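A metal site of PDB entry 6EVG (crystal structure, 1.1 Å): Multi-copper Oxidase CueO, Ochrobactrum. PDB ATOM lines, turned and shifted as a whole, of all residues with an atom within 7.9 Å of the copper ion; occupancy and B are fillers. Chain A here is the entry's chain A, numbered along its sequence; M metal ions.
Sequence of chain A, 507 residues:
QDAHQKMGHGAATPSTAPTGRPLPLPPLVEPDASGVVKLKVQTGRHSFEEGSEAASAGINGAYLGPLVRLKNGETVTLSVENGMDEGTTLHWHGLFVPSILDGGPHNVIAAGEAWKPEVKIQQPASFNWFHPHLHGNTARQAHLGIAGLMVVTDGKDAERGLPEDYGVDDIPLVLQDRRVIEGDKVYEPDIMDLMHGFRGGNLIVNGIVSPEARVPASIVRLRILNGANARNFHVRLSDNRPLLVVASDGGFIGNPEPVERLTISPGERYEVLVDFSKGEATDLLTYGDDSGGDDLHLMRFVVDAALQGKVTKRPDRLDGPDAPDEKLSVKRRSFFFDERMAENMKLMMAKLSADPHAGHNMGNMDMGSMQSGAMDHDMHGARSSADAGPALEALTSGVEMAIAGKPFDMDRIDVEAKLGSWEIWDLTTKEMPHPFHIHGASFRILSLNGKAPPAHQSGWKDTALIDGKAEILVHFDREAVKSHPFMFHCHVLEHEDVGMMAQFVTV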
ATOM      1  N   LEU A 194       0.632 -38.383   2.717  1.00  0.00           N
ATOM      2  CA  LEU A 194       0.772 -36.971   2.282  1.00  0.00           C
ATOM      3  C   LEU A 194      -0.419 -36.159   2.819  1.00  0.00           C
ATOM      4  O   LEU A 194      -0.271 -34.992   3.199  1.00  0.00           O
ATOM      5  CB  LEU A 194       0.856 -36.847   0.768  1.00  0.00           C
ATOM      6  CG  LEU A 194       2.094 -37.439   0.152  1.00  0.00           C
ATOM      7  CD1 LEU A 194       2.064 -37.271  -1.383  1.00  0.00           C
ATOM      8  CD2 LEU A 194       3.398 -36.883   0.763  1.00  0.00           C
ATOM      9  N   MET A 195      -1.637 -36.759   2.814  1.00  0.00           N
ATOM     10  CA  MET A 195      -2.822 -36.027   3.273  1.00  0.00           C
ATOM     11  C   MET A 195      -2.840 -35.853   4.778  1.00  0.00           C
ATOM     12  O   MET A 195      -3.233 -34.764   5.276  1.00  0.00           O
ATOM     13  CB  MET A 195      -4.075 -36.686   2.809  1.00  0.00           C
ATOM     14  CG  MET A 195      -4.274 -36.581   1.299  1.00  0.00           C
ATOM     15  SD  MET A 195      -5.744 -37.297   0.627  1.00  0.00           S
ATOM     16  CE  MET A 195      -6.919 -36.168   1.322  1.00  0.00           C
ATOM     17  N   HIS A 196      -2.404 -36.827   5.541  1.00  0.00           N
ATOM     18  CA  HIS A 196      -2.617 -36.843   7.019  1.00  0.00           C
ATOM     19  C   HIS A 196      -1.341 -36.710   7.819  1.00  0.00           C
ATOM     20  O   HIS A 196      -1.443 -36.567   9.036  1.00  0.00           O
ATOM     21  CB  HIS A 196      -3.421 -38.090   7.446  1.00  0.00           C
ATOM     22  CG  HIS A 196      -4.787 -38.128   6.810  1.00  0.00           C
ATOM     23  ND1 HIS A 196      -5.789 -37.241   7.146  1.00  0.00           N
ATOM     24  CD2 HIS A 196      -5.270 -38.839   5.777  1.00  0.00           C
ATOM     25  CE1 HIS A 196      -6.870 -37.471   6.402  1.00  0.00           C
ATOM     26  NE2 HIS A 196      -6.578 -38.473   5.578  1.00  0.00           N
ATOM     27  N   GLY A 197      -0.195 -36.777   7.149  1.00  0.00           N
ATOM     28  CA  GLY A 197       1.102 -36.829   7.826  1.00  0.00           C
ATOM     29  C   GLY A 197       1.593 -38.259   7.954  1.00  0.00           C
ATOM     30  O   GLY A 197       0.806 -39.180   8.110  1.00  0.00           O
ATOM     31  N   PHE A 337      -5.311 -23.336   7.475  1.00  0.00           N
ATOM     32  CA  PHE A 337      -4.593 -24.509   7.043  1.00  0.00           C
ATOM     33  C   PHE A 337      -5.509 -25.344   6.134  1.00  0.00           C
ATOM     34  O   PHE A 337      -6.338 -26.140   6.599  1.00  0.00           O
ATOM     35  CB  PHE A 337      -4.150 -25.342   8.271  1.00  0.00           C
ATOM     36  CG  PHE A 337      -3.102 -24.679   9.129  1.00  0.00           C
ATOM     37  CD1 PHE A 337      -3.404 -23.749  10.082  1.00  0.00           C
ATOM     38  CD2 PHE A 337      -1.763 -24.964   8.948  1.00  0.00           C
ATOM     39  CE1 PHE A 337      -2.404 -23.209  10.888  1.00  0.00           C
ATOM     40  CE2 PHE A 337      -0.793 -24.392   9.721  1.00  0.00           C
ATOM     41  CZ  PHE A 337      -1.114 -23.503  10.676  1.00  0.00           C
ATOM     42  N   ASP A 338      -5.354 -25.104   4.840  1.00  0.00           N
ATOM     43  CA  ASP A 338      -6.259 -25.649   3.861  1.00  0.00           C
ATOM     44  C   ASP A 338      -5.692 -26.953   3.313  1.00  0.00           C
ATOM     45  O   ASP A 338      -4.768 -26.967   2.463  1.00  0.00           O
ATOM     46  CB  ASP A 338      -6.474 -24.622   2.742  1.00  0.00           C
ATOM     47  CG  ASP A 338      -7.631 -24.992   1.840  1.00  0.00           C
ATOM     48  OD1 ASP A 338      -8.145 -26.119   1.875  1.00  0.00           O
ATOM     49  OD2 ASP A 338      -8.068 -24.067   1.087  1.00  0.00           O
ATOM     50  N   GLU A 339      -6.272 -28.067   3.757  1.00  0.00           N
ATOM     51  CA  GLU A 339      -5.865 -29.393   3.346  1.00  0.00           C
ATOM     52  C   GLU A 339      -6.388 -29.747   1.943  1.00  0.00           C
ATOM     53  O   GLU A 339      -5.971 -30.747   1.401  1.00  0.00           O
ATOM     54  CB  GLU A 339      -6.377 -30.444   4.330  1.00  0.00           C
ATOM     55  CG  GLU A 339      -5.790 -30.264   5.723  1.00  0.00           C
ATOM     56  CD  GLU A 339      -6.469 -31.110   6.830  1.00  0.00           C
ATOM     57  OE1 GLU A 339      -6.724 -32.304   6.571  1.00  0.00           O
ATOM     58  OE2 GLU A 339      -6.715 -30.541   7.994  1.00  0.00           O
ATOM     59  N   MET A 401      -1.732 -28.410  -0.966  1.00  0.00           N
ATOM     60  CA  MET A 401      -2.352 -27.772   0.194  1.00  0.00           C
ATOM     61  C   MET A 401      -1.881 -26.332   0.221  1.00  0.00           C
ATOM     62  O   MET A 401      -0.977 -25.899  -0.553  1.00  0.00           O
ATOM     63  CB  MET A 401      -1.959 -28.518   1.476  1.00  0.00           C
ATOM     64  CG  MET A 401      -2.470 -29.890   1.517  1.00  0.00           C
ATOM     65  SD  MET A 401      -2.071 -30.693   3.099  1.00  0.00           S
ATOM     66  CE  MET A 401      -2.649 -32.296   2.770  1.00  0.00           C
ATOM     67  N   ALA A 402      -2.401 -25.548   1.133  1.00  0.00           N
ATOM     68  CA  ALA A 402      -2.072 -24.130   1.235  1.00  0.00           C
ATOM     69  C   ALA A 402      -2.218 -23.652   2.651  1.00  0.00           C
ATOM     70  O   ALA A 402      -3.049 -24.150   3.439  1.00  0.00           O
ATOM     71  CB  ALA A 402      -2.967 -23.272   0.341  1.00  0.00           C
ATOM     72  N   ILE A 403      -1.427 -22.647   3.015  1.00  0.00           N
ATOM     73  CA  ILE A 403      -1.607 -21.851   4.209  1.00  0.00           C
ATOM     74  C   ILE A 403      -2.025 -20.396   3.928  1.00  0.00           C
ATOM     75  O   ILE A 403      -2.729 -19.768   4.722  1.00  0.00           O
ATOM     76  CB  ILE A 403      -0.371 -21.908   5.173  1.00  0.00           C
ATOM     77  CG1 ILE A 403      -0.701 -21.414   6.590  1.00  0.00           C
ATOM     78  CG2 ILE A 403       0.844 -21.210   4.614  1.00  0.00           C
ATOM     79  CD1 ILE A 403       0.396 -21.741   7.586  1.00  0.00           C
ATOM     80  N   THR A 429      -7.953 -24.200  11.752  1.00  0.00           N
ATOM     81  CA  THR A 429      -7.894 -25.530  11.153  1.00  0.00           C
ATOM     82  C   THR A 429      -9.315 -26.097  11.009  1.00  0.00           C
ATOM     83  O   THR A 429     -10.252 -25.621  11.619  1.00  0.00           O
ATOM     84  CB  THR A 429      -7.022 -26.498  11.977  1.00  0.00           C
ATOM     85  OG1 THR A 429      -7.661 -26.736  13.243  1.00  0.00           O
ATOM     86  CG2 THR A 429      -5.661 -25.934  12.240  1.00  0.00           C
ATOM     87  N   MET A 432      -8.025 -31.610  10.869  1.00  0.00           N
ATOM     88  CA  MET A 432      -7.021 -32.098  11.849  1.00  0.00           C
ATOM     89  C   MET A 432      -6.270 -30.914  12.418  1.00  0.00           C
ATOM     90  O   MET A 432      -6.295 -29.833  11.826  1.00  0.00           O
ATOM     91  CB  MET A 432      -6.076 -33.128  11.245  1.00  0.00           C
ATOM     92  CG  MET A 432      -5.135 -32.559  10.171  1.00  0.00           C
ATOM     93  SD  MET A 432      -3.989 -33.783   9.480  1.00  0.00           S
ATOM     94  CE  MET A 432      -2.702 -33.900  10.699  1.00  0.00           C
ATOM     95  N   PRO A 433      -5.554 -31.100  13.535  1.00  0.00           N
ATOM     96  CA  PRO A 433      -4.710 -30.037  14.055  1.00  0.00           C
ATOM     97  C   PRO A 433      -3.431 -29.882  13.204  1.00  0.00           C
ATOM     98  O   PRO A 433      -3.030 -30.846  12.553  1.00  0.00           O
ATOM     99  CB  PRO A 433      -4.338 -30.535  15.441  1.00  0.00           C
ATOM    100  CG  PRO A 433      -4.930 -31.855  15.640  1.00  0.00           C
ATOM    101  CD  PRO A 433      -5.551 -32.286  14.397  1.00  0.00           C
ATOM    102  N   HIS A 434      -2.863 -28.677  13.247  1.00  0.00           N
ATOM    103  CA  HIS A 434      -1.620 -28.410  12.489  1.00  0.00           C
ATOM    104  C   HIS A 434      -0.668 -27.623  13.334  1.00  0.00           C
ATOM    105  O   HIS A 434      -1.057 -26.623  13.942  1.00  0.00           O
ATOM    106  CB  HIS A 434      -1.900 -27.607  11.196  1.00  0.00           C
ATOM    107  CG  HIS A 434      -2.783 -28.308  10.211  1.00  0.00           C
ATOM    108  ND1 HIS A 434      -2.303 -29.023   9.125  1.00  0.00           N
ATOM    109  CD2 HIS A 434      -4.141 -28.425  10.171  1.00  0.00           C
ATOM    110  CE1 HIS A 434      -3.324 -29.537   8.481  1.00  0.00           C
ATOM    111  NE2 HIS A 434      -4.444 -29.211   9.095  1.00  0.00           N
ATOM    112  N   PRO A 435       0.626 -28.010  13.375  1.00  0.00           N
ATOM    113  CA  PRO A 435       1.646 -27.176  14.071  1.00  0.00           C
ATOM    114  C   PRO A 435       2.119 -26.031  13.174  1.00  0.00           C
ATOM    115  O   PRO A 435       2.737 -26.217  12.174  1.00  0.00           O
ATOM    116  CB  PRO A 435       2.730 -28.197  14.348  1.00  0.00           C
ATOM    117  CG  PRO A 435       2.635 -29.197  13.230  1.00  0.00           C
ATOM    118  CD  PRO A 435       1.147 -29.272  12.883  1.00  0.00           C
ATOM    119  N   PHE A 436       1.848 -24.817  13.600  1.00  0.00           N
ATOM    120  CA  PHE A 436       2.315 -23.610  12.933  1.00  0.00           C
ATOM    121  C   PHE A 436       3.750 -23.305  13.336  1.00  0.00           C
ATOM    122  O   PHE A 436       4.031 -23.252  14.520  1.00  0.00           O
ATOM    123  CB  PHE A 436       1.424 -22.454  13.388  1.00  0.00           C
ATOM    124  CG  PHE A 436       1.864 -21.096  12.903  1.00  0.00           C
ATOM    125  CD1 PHE A 436       1.550 -20.692  11.610  1.00  0.00           C
ATOM    126  CD2 PHE A 436       2.526 -20.205  13.698  1.00  0.00           C
ATOM    127  CE1 PHE A 436       1.921 -19.423  11.191  1.00  0.00           C
ATOM    128  CE2 PHE A 436       2.898 -18.975  13.292  1.00  0.00           C
ATOM    129  CZ  PHE A 436       2.616 -18.571  11.983  1.00  0.00           C
ATOM    130  N   HIS A 489       4.703 -21.883   7.961  1.00  0.00           N
ATOM    131  CA  HIS A 489       4.231 -23.129   7.400  1.00  0.00           C
ATOM    132  C   HIS A 489       3.681 -24.036   8.484  1.00  0.00           C
ATOM    133  O   HIS A 489       3.920 -23.838   9.659  1.00  0.00           O
ATOM    134  CB  HIS A 489       5.365 -23.845   6.601  1.00  0.00           C
ATOM    135  CG  HIS A 489       6.612 -24.109   7.394  1.00  0.00           C
ATOM    136  ND1 HIS A 489       6.827 -25.289   8.049  1.00  0.00           N
ATOM    137  CD2 HIS A 489       7.715 -23.362   7.610  1.00  0.00           C
ATOM    138  CE1 HIS A 489       8.021 -25.238   8.633  1.00  0.00           C
ATOM    139  NE2 HIS A 489       8.561 -24.057   8.424  1.00  0.00           N
ATOM    140  N   CYS A 490       3.056 -25.119   8.007  1.00  0.00           N
ATOM    141  CA  CYS A 490       2.753 -26.266   8.850  1.00  0.00           C
ATOM    142  C   CYS A 490       4.031 -27.055   9.022  1.00  0.00           C
ATOM    143  O   CYS A 490       4.802 -27.255   8.088  1.00  0.00           O
ATOM    144  CB  CYS A 490       1.664 -27.101   8.245  1.00  0.00           C
ATOM    145  SG  CYS A 490       1.236 -28.512   9.288  1.00  0.00           S
ATOM    146  N   HIS A 491       4.251 -27.558  10.254  1.00  0.00           N
ATOM    147  CA  HIS A 491       5.381 -28.402  10.585  1.00  0.00           C
ATOM    148  C   HIS A 491       5.105 -29.919  10.512  1.00  0.00           C
ATOM    149  O   HIS A 491       5.985 -30.692  10.879  1.00  0.00           O
ATOM    150  CB  HIS A 491       6.027 -27.986  11.935  1.00  0.00           C
ATOM    151  CG  HIS A 491       7.517 -28.048  11.969  1.00  0.00           C
ATOM    152  ND1 HIS A 491       8.264 -29.191  11.960  1.00  0.00           N
ATOM    153  CD2 HIS A 491       8.424 -27.013  11.930  1.00  0.00           C
ATOM    154  CE1 HIS A 491       9.575 -28.847  11.926  1.00  0.00           C
ATOM    155  NE2 HIS A 491       9.693 -27.542  11.928  1.00  0.00           N
ATOM    156  N   VAL A 492       3.919 -30.299   9.974  1.00  0.00           N
ATOM    157  CA  VAL A 492       3.755 -31.646   9.451  1.00  0.00           C
ATOM    158  C   VAL A 492       4.485 -31.651   8.113  1.00  0.00           C
ATOM    159  O   VAL A 492       4.103 -30.942   7.212  1.00  0.00           O
ATOM    160  CB  VAL A 492       2.258 -32.030   9.301  1.00  0.00           C
ATOM    161  CG1 VAL A 492       2.097 -33.322   8.530  1.00  0.00           C
ATOM    162  CG2 VAL A 492       1.651 -32.184  10.669  1.00  0.00           C
ATOM    163  N   LEU A 493       5.583 -32.383   8.047  1.00  0.00           N
ATOM    164  CA  LEU A 493       6.515 -32.163   6.942  1.00  0.00           C
ATOM    165  C   LEU A 493       5.906 -32.536   5.603  1.00  0.00           C
ATOM    166  O   LEU A 493       6.225 -31.906   4.564  1.00  0.00           O
ATOM    167  CB  LEU A 493       7.809 -32.901   7.198  1.00  0.00           C
ATOM    168  CG  LEU A 493       8.530 -32.496   8.482  1.00  0.00           C
ATOM    169  CD1 LEU A 493       9.865 -33.235   8.558  1.00  0.00           C
ATOM    170  CD2 LEU A 493       8.744 -30.996   8.549  1.00  0.00           C
ATOM    171  N   GLU A 494       5.025 -33.536   5.570  1.00  0.00           N
ATOM    172  CA  GLU A 494       4.300 -33.854   4.344  1.00  0.00           C
ATOM    173  C   GLU A 494       3.459 -32.674   3.849  1.00  0.00           C
ATOM    174  O   GLU A 494       3.399 -32.391   2.641  1.00  0.00           O
ATOM    175  CB  GLU A 494       3.418 -35.077   4.562  1.00  0.00           C
ATOM    176  CG  GLU A 494       4.196 -36.357   4.714  1.00  0.00           C
ATOM    177  CD  GLU A 494       5.048 -36.459   5.960  1.00  0.00           C
ATOM    178  OE1 GLU A 494       4.542 -36.108   7.062  1.00  0.00           O
ATOM    179  OE2 GLU A 494       6.211 -36.928   5.838  1.00  0.00           O
ATOM    180  N   HIS A 495       2.827 -31.964   4.782  1.00  0.00           N
ATOM    181  CA  HIS A 495       1.940 -30.835   4.437  1.00  0.00           C
ATOM    182  C   HIS A 495       2.801 -29.707   3.868  1.00  0.00           C
ATOM    183  O   HIS A 495       2.424 -29.087   2.861  1.00  0.00           O
ATOM    184  CB  HIS A 495       1.148 -30.365   5.638  1.00  0.00           C
ATOM    185  CG  HIS A 495       0.125 -31.342   6.080  1.00  0.00           C
ATOM    186  ND1 HIS A 495      -0.593 -31.067   7.236  1.00  0.00           N
ATOM    187  CD2 HIS A 495      -0.309 -32.519   5.549  1.00  0.00           C
ATOM    188  CE1 HIS A 495      -1.470 -32.068   7.339  1.00  0.00           C
ATOM    189  NE2 HIS A 495      -1.297 -32.962   6.365  1.00  0.00           N
ATOM    190  N   GLU A 496       3.897 -29.385   4.539  1.00  0.00           N
ATOM    191  CA  GLU A 496       4.812 -28.355   4.022  1.00  0.00           C
ATOM    192  C   GLU A 496       5.284 -28.736   2.579  1.00  0.00           C
ATOM    193  O   GLU A 496       5.304 -27.898   1.694  1.00  0.00           O
ATOM    194  CB  GLU A 496       6.002 -28.324   4.983  1.00  0.00           C
ATOM    195  CG  GLU A 496       7.066 -27.345   4.675  1.00  0.00           C
ATOM    196  CD  GLU A 496       8.293 -27.640   5.554  1.00  0.00           C
ATOM    197  OE1 GLU A 496       8.196 -27.847   6.737  1.00  0.00           O
ATOM    198  OE2 GLU A 496       9.254 -27.697   4.955  1.00  0.00           O
ATOM    199  N   MET A 500       1.794 -26.376   2.007  1.00  0.00           N
ATOM    200  CA  MET A 500       1.267 -25.643   3.154  1.00  0.00           C
ATOM    201  C   MET A 500       2.359 -24.774   3.807  1.00  0.00           C
ATOM    202  O   MET A 500       2.842 -25.000   4.928  1.00  0.00           O
ATOM    203  CB  MET A 500       0.687 -26.649   4.145  1.00  0.00           C
ATOM    204  CG  MET A 500      -0.168 -26.043   5.178  1.00  0.00           C
ATOM    205  SD  MET A 500      -1.193 -27.208   6.167  1.00  0.00           S
ATOM    206  CE  MET A 500      -2.599 -27.526   5.213  1.00  0.00           C
HETATM  207 CU    CU M   1      -0.492 -29.495   8.457  1.00  0.00          CU
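Merely in contact with the copper ion: Val 492 and Met 500.
Of the 25 residues printed, 5 come within 4 Å of the copper ion.
The nearest printed residue that does not touch the copper ion is Pro 435 (4.7 Å).
A ring nitrogen (ND1) of His 434 sits close to the side-chain sulfur (SD) of Met 500 (3.6 Å).
A ring nitrogen (NE2) of His 434 lies close to the backbone carbonyl oxygen of Met 432.
NE2 of His 434 lies within hydrogen-bond range of OE2 of Glu 339 (2.9 Å).
The backbone carbonyl oxygen (O) of His 495 is in hydrogen-bond range of the backbone NH (N) of Met 500, 2.9 Å away.
O of Met 195 is in hydrogen-bond range of NE2 of His 495, 2.9 Å away.
O of Met 500 is in hydrogen-bond range of N of Cys 490, 3.1 Å away.
SG of Cys 490 sits close to N of Val 492 (3.3 Å).
A ring nitrogen (ND1) of His 434 is bound to the copper ion (2.0 Å).
ND1 of His 495 binds the copper ion.
The copper ion is bound by SG of Cys 490 (2.2 Å).
The copper ion has three donor atoms within binding distance.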
